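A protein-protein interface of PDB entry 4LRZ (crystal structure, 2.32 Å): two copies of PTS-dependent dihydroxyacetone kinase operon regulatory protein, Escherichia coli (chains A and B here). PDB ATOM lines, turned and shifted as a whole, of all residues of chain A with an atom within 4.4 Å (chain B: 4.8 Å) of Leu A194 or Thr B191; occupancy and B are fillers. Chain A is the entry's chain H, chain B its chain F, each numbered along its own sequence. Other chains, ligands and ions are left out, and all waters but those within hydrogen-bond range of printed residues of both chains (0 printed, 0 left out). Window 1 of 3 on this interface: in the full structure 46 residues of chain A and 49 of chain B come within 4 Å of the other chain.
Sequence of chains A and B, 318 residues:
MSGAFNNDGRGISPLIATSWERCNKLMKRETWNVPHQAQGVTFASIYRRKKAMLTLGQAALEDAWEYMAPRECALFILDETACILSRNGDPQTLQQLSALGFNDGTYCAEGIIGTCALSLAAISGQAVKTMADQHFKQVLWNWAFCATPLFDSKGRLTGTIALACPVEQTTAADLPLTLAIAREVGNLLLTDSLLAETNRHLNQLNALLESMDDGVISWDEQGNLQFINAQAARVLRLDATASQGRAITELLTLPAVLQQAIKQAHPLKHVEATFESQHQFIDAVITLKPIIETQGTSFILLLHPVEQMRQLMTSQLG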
ATOM      1  N   LEU A 190      -6.723 -15.738 -11.710  1.00  0.00           N
ATOM      2  CA  LEU A 190      -7.353 -14.736 -10.905  1.00  0.00           C
ATOM      3  C   LEU A 190      -6.500 -13.469 -10.810  1.00  0.00           C
ATOM      4  O   LEU A 190      -7.039 -12.368 -10.861  1.00  0.00           O
ATOM      5  CB  LEU A 190      -7.649 -15.310  -9.520  1.00  0.00           C
ATOM      6  CG  LEU A 190      -8.317 -14.366  -8.530  1.00  0.00           C
ATOM      7  CD1 LEU A 190      -9.731 -14.111  -9.054  1.00  0.00           C
ATOM      8  CD2 LEU A 190      -8.342 -14.959  -7.111  1.00  0.00           C
ATOM      9  N   THR A 191      -5.185 -13.619 -10.669  1.00  0.00           N
ATOM     10  CA  THR A 191      -4.325 -12.454 -10.522  1.00  0.00           C
ATOM     11  C   THR A 191      -4.250 -11.737 -11.854  1.00  0.00           C
ATOM     12  O   THR A 191      -4.219 -10.521 -11.880  1.00  0.00           O
ATOM     13  CB  THR A 191      -2.902 -12.750  -9.957  1.00  0.00           C
ATOM     14  OG1 THR A 191      -2.005 -13.143 -11.003  1.00  0.00           O
ATOM     15  CG2 THR A 191      -2.946 -13.842  -8.977  1.00  0.00           C
ATOM     16  N   ASP A 192      -4.265 -12.474 -12.962  1.00  0.00           N
ATOM     17  CA  ASP A 192      -4.408 -11.794 -14.260  1.00  0.00           C
ATOM     18  C   ASP A 192      -5.647 -10.924 -14.298  1.00  0.00           C
ATOM     19  O   ASP A 192      -5.629  -9.804 -14.823  1.00  0.00           O
ATOM     20  CB  ASP A 192      -4.375 -12.751 -15.475  1.00  0.00           C
ATOM     21  CG  ASP A 192      -2.918 -13.162 -15.880  1.00  0.00           C
ATOM     22  OD1 ASP A 192      -1.979 -12.338 -15.700  1.00  0.00           O
ATOM     23  OD2 ASP A 192      -2.696 -14.299 -16.364  1.00  0.00           O
ATOM     24  N   SER A 193      -6.733 -11.411 -13.734  1.00  0.00           N
ATOM     25  CA  SER A 193      -7.966 -10.637 -13.835  1.00  0.00           C
ATOM     26  C   SER A 193      -8.027  -9.440 -12.855  1.00  0.00           C
ATOM     27  O   SER A 193      -8.552  -8.401 -13.200  1.00  0.00           O
ATOM     28  CB  SER A 193      -9.210 -11.534 -13.891  1.00  0.00           C
ATOM     29  OG  SER A 193      -9.918 -11.592 -12.676  1.00  0.00           O
ATOM     30  N   LEU A 194      -7.362  -9.550 -11.698  1.00  0.00           N
ATOM     31  CA  LEU A 194      -7.271  -8.415 -10.732  1.00  0.00           C
ATOM     32  C   LEU A 194      -6.522  -7.262 -11.312  1.00  0.00           C
ATOM     33  O   LEU A 194      -6.949  -6.139 -11.186  1.00  0.00           O
ATOM     34  CB  LEU A 194      -6.647  -8.843  -9.396  1.00  0.00           C
ATOM     35  CG  LEU A 194      -7.436  -9.933  -8.696  1.00  0.00           C
ATOM     36  CD1 LEU A 194      -6.631 -10.628  -7.582  1.00  0.00           C
ATOM     37  CD2 LEU A 194      -8.806  -9.383  -8.232  1.00  0.00           C
ATOM     38  N   LEU A 195      -5.389  -7.539 -11.949  1.00  0.00           N
ATOM     39  CA  LEU A 195      -4.624  -6.532 -12.697  1.00  0.00           C
ATOM     40  C   LEU A 195      -5.431  -5.823 -13.799  1.00  0.00           C
ATOM     41  O   LEU A 195      -5.333  -4.612 -13.950  1.00  0.00           O
ATOM     42  CB  LEU A 195      -3.414  -7.215 -13.340  1.00  0.00           C
ATOM     43  CG  LEU A 195      -2.192  -7.536 -12.479  1.00  0.00           C
ATOM     44  CD1 LEU A 195      -1.326  -8.587 -13.190  1.00  0.00           C
ATOM     45  CD2 LEU A 195      -1.399  -6.231 -12.179  1.00  0.00           C
ATOM     46  N   ALA A 196      -6.202  -6.570 -14.582  1.00  0.00           N
ATOM     47  CA  ALA A 196      -7.157  -5.964 -15.531  1.00  0.00           C
ATOM     48  C   ALA A 196      -8.167  -5.058 -14.816  1.00  0.00           C
ATOM     49  O   ALA A 196      -8.405  -3.892 -15.244  1.00  0.00           O
ATOM     50  CB  ALA A 196      -7.900  -7.038 -16.362  1.00  0.00           C
ATOM     51  N   GLU A 197      -8.748  -5.556 -13.723  1.00  0.00           N
ATOM     52  CA  GLU A 197      -9.696  -4.727 -12.948  1.00  0.00           C
ATOM     53  C   GLU A 197      -9.021  -3.450 -12.447  1.00  0.00           C
ATOM     54  O   GLU A 197      -9.547  -2.351 -12.606  1.00  0.00           O
ATOM     55  CB  GLU A 197     -10.375  -5.538 -11.819  1.00  0.00           C
ATOM     56  CG  GLU A 197     -11.166  -6.781 -12.411  1.00  0.00           C
ATOM     57  CD  GLU A 197     -12.235  -7.440 -11.486  1.00  0.00           C
ATOM     58  OE1 GLU A 197     -12.116  -8.666 -11.207  1.00  0.00           O
ATOM     59  OE2 GLU A 197     -13.210  -6.743 -11.079  1.00  0.00           O
ATOM     60  N   THR A 198      -7.822  -3.569 -11.880  1.00  0.00           N
ATOM     61  CA  THR A 198      -7.132  -2.360 -11.511  1.00  0.00           C
ATOM     62  C   THR A 198      -6.822  -1.433 -12.688  1.00  0.00           C
ATOM     63  O   THR A 198      -7.003  -0.238 -12.571  1.00  0.00           O
ATOM     64  CB  THR A 198      -5.936  -2.551 -10.536  1.00  0.00           C
ATOM     65  OG1 THR A 198      -4.949  -1.524 -10.767  1.00  0.00           O
ATOM     66  CG2 THR A 198      -5.333  -3.777 -10.722  1.00  0.00           C
ATOM     67  N   ASN B 187       1.636 -16.918  -4.408  1.00  0.00           N
ATOM     68  CA  ASN B 187       0.766 -16.181  -5.286  1.00  0.00           C
ATOM     69  C   ASN B 187      -0.461 -15.647  -4.559  1.00  0.00           C
ATOM     70  O   ASN B 187      -1.004 -14.610  -4.941  1.00  0.00           O
ATOM     71  CB  ASN B 187       0.422 -16.995  -6.523  1.00  0.00           C
ATOM     72  CG  ASN B 187       1.626 -17.197  -7.418  1.00  0.00           C
ATOM     73  OD1 ASN B 187       2.529 -16.354  -7.464  1.00  0.00           O
ATOM     74  ND2 ASN B 187       1.672 -18.318  -8.097  1.00  0.00           N
ATOM     75  N   LEU B 188      -0.860 -16.340  -3.501  1.00  0.00           N
ATOM     76  CA  LEU B 188      -1.980 -15.889  -2.745  1.00  0.00           C
ATOM     77  C   LEU B 188      -1.620 -14.618  -1.978  1.00  0.00           C
ATOM     78  O   LEU B 188      -2.478 -13.782  -1.773  1.00  0.00           O
ATOM     79  CB  LEU B 188      -2.435 -16.960  -1.811  1.00  0.00           C
ATOM     80  CG  LEU B 188      -3.657 -17.844  -2.075  1.00  0.00           C
ATOM     81  CD1 LEU B 188      -4.522 -17.523  -3.258  1.00  0.00           C
ATOM     82  CD2 LEU B 188      -3.276 -19.319  -1.956  1.00  0.00           C
ATOM     83  N   LEU B 189      -0.363 -14.474  -1.558  1.00  0.00           N
ATOM     84  CA  LEU B 189       0.058 -13.249  -0.883  1.00  0.00           C
ATOM     85  C   LEU B 189       0.037 -12.132  -1.906  1.00  0.00           C
ATOM     86  O   LEU B 189      -0.398 -11.024  -1.620  1.00  0.00           O
ATOM     87  CB  LEU B 189       1.440 -13.366  -0.244  1.00  0.00           C
ATOM     88  CG  LEU B 189       1.548 -14.311   0.971  1.00  0.00           C
ATOM     89  CD1 LEU B 189       3.031 -14.570   1.300  1.00  0.00           C
ATOM     90  CD2 LEU B 189       0.809 -13.788   2.206  1.00  0.00           C
ATOM     91  N   LEU B 190       0.464 -12.437  -3.111  1.00  0.00           N
ATOM     92  CA  LEU B 190       0.375 -11.487  -4.203  1.00  0.00           C
ATOM     93  C   LEU B 190      -1.064 -11.050  -4.540  1.00  0.00           C
ATOM     94  O   LEU B 190      -1.293  -9.849  -4.830  1.00  0.00           O
ATOM     95  CB  LEU B 190       1.038 -12.093  -5.441  1.00  0.00           C
ATOM     96  CG  LEU B 190       1.019 -11.263  -6.715  1.00  0.00           C
ATOM     97  CD1 LEU B 190       1.951 -10.096  -6.525  1.00  0.00           C
ATOM     98  CD2 LEU B 190       1.489 -12.146  -7.898  1.00  0.00           C
ATOM     99  N   THR B 191      -2.025 -11.984  -4.491  1.00  0.00           N
ATOM    100  CA  THR B 191      -3.394 -11.589  -4.792  1.00  0.00           C
ATOM    101  C   THR B 191      -3.982 -10.727  -3.663  1.00  0.00           C
ATOM    102  O   THR B 191      -4.689  -9.788  -3.958  1.00  0.00           O
ATOM    103  CB  THR B 191      -4.364 -12.741  -5.222  1.00  0.00           C
ATOM    104  OG1 THR B 191      -4.893 -13.388  -4.071  1.00  0.00           O
ATOM    105  CG2 THR B 191      -3.676 -13.770  -6.066  1.00  0.00           C
ATOM    106  N   ASP B 192      -3.639 -11.004  -2.400  1.00  0.00           N
ATOM    107  CA  ASP B 192      -4.016 -10.103  -1.280  1.00  0.00           C
ATOM    108  C   ASP B 192      -3.487  -8.689  -1.538  1.00  0.00           C
ATOM    109  O   ASP B 192      -4.192  -7.689  -1.336  1.00  0.00           O
ATOM    110  CB  ASP B 192      -3.488 -10.590   0.086  1.00  0.00           C
ATOM    111  CG  ASP B 192      -4.404 -11.643   0.761  1.00  0.00           C
ATOM    112  OD1 ASP B 192      -5.527 -11.897   0.265  1.00  0.00           O
ATOM    113  OD2 ASP B 192      -4.000 -12.236   1.794  1.00  0.00           O
ATOM    114  N   SER B 193      -2.246  -8.603  -1.993  1.00  0.00           N
ATOM    115  CA  SER B 193      -1.643  -7.291  -2.194  1.00  0.00           C
ATOM    116  C   SER B 193      -2.192  -6.574  -3.450  1.00  0.00           C
ATOM    117  O   SER B 193      -2.318  -5.364  -3.463  1.00  0.00           O
ATOM    118  CB  SER B 193      -0.119  -7.371  -2.134  1.00  0.00           C
ATOM    119  OG  SER B 193       0.461  -7.429  -3.412  1.00  0.00           O
ATOM    120  N   LEU B 194      -2.631  -7.336  -4.452  1.00  0.00           N
ATOM    121  CA  LEU B 194      -3.252  -6.725  -5.637  1.00  0.00           C
ATOM    122  C   LEU B 194      -4.595  -6.077  -5.294  1.00  0.00           C
ATOM    123  O   LEU B 194      -4.883  -5.001  -5.770  1.00  0.00           O
ATOM    124  CB  LEU B 194      -3.398  -7.732  -6.783  1.00  0.00           C
ATOM    125  CG  LEU B 194      -2.076  -8.171  -7.391  1.00  0.00           C
ATOM    126  CD1 LEU B 194      -2.235  -9.424  -8.266  1.00  0.00           C
ATOM    127  CD2 LEU B 194      -1.416  -7.034  -8.160  1.00  0.00           C
ATOM    128  N   LEU B 195      -5.384  -6.756  -4.470  1.00  0.00           N
ATOM    129  CA  LEU B 195      -6.670  -6.276  -3.982  1.00  0.00           C
ATOM    130  C   LEU B 195      -6.490  -5.034  -3.108  1.00  0.00           C
ATOM    131  O   LEU B 195      -7.202  -4.050  -3.259  1.00  0.00           O
ATOM    132  CB  LEU B 195      -7.387  -7.389  -3.221  1.00  0.00           C
ATOM    133  CG  LEU B 195      -8.169  -8.459  -4.018  1.00  0.00           C
ATOM    134  CD1 LEU B 195      -8.437  -9.752  -3.177  1.00  0.00           C
ATOM    135  CD2 LEU B 195      -9.495  -7.897  -4.570  1.00  0.00           C
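Of the 9 printed residues of chain B, 2 touch a printed residue of chain A.
Hydrophobic or aromatic side chains of chain B that line the printed part of chain A: Leu B194.
Printed residues of chain A that touch a printed residue of chain B: Thr A191 and Leu A194.
Hydrophobic or aromatic side chains of chain A within 4 Å of the printed part of chain B: Leu A194.
Along chain A the printed residues that touch a printed residue of chain B span positions 191 to 194.
Among the printed residues, no Asp or Glu carboxylate lies within 4 Å of a Lys or Arg side-chain nitrogen of the other chain.
O of Leu B188 lies within hydrogen-bond range of OG1 of Thr B191 (3.4 Å).
Thr B191 touches its own counterpart, Thr A191.
Thr A191 touches Leu B194, and with the chains exchanged Leu A194 touches Thr B191.
Of the 3 pairs that touch across the chains among the printed residues, 3 have their exchanged pair printed and touching as well.
Of the printed residues of chain B, Thr A191 touches Thr B191 (3.0 Å) and Leu B194 (3.8 Å).
Thr B191 touches just these residues of chain A: Thr A191 and Leu A194.
Of the printed residues of chain A, Leu B194 touches Thr A191.
The nearest printed residue of chain B that does not touch Leu A194 is Leu B195 (4.01 Å).
The nearest printed residue of chain A that does not touch Thr B191 is Leu A190 (4.9 Å).
The nearest printed residue of chain A that does not touch Leu B194 is Leu A195 (4.1 Å).
Thr A191 touches Thr B191 (CG2 to CG2, 3.0 Å).
Thr A191 touches Leu B194 (CB to CD1, 3.8 Å).
CD1 of Leu A194 touches CB of Thr B191, 3.9 Å away.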
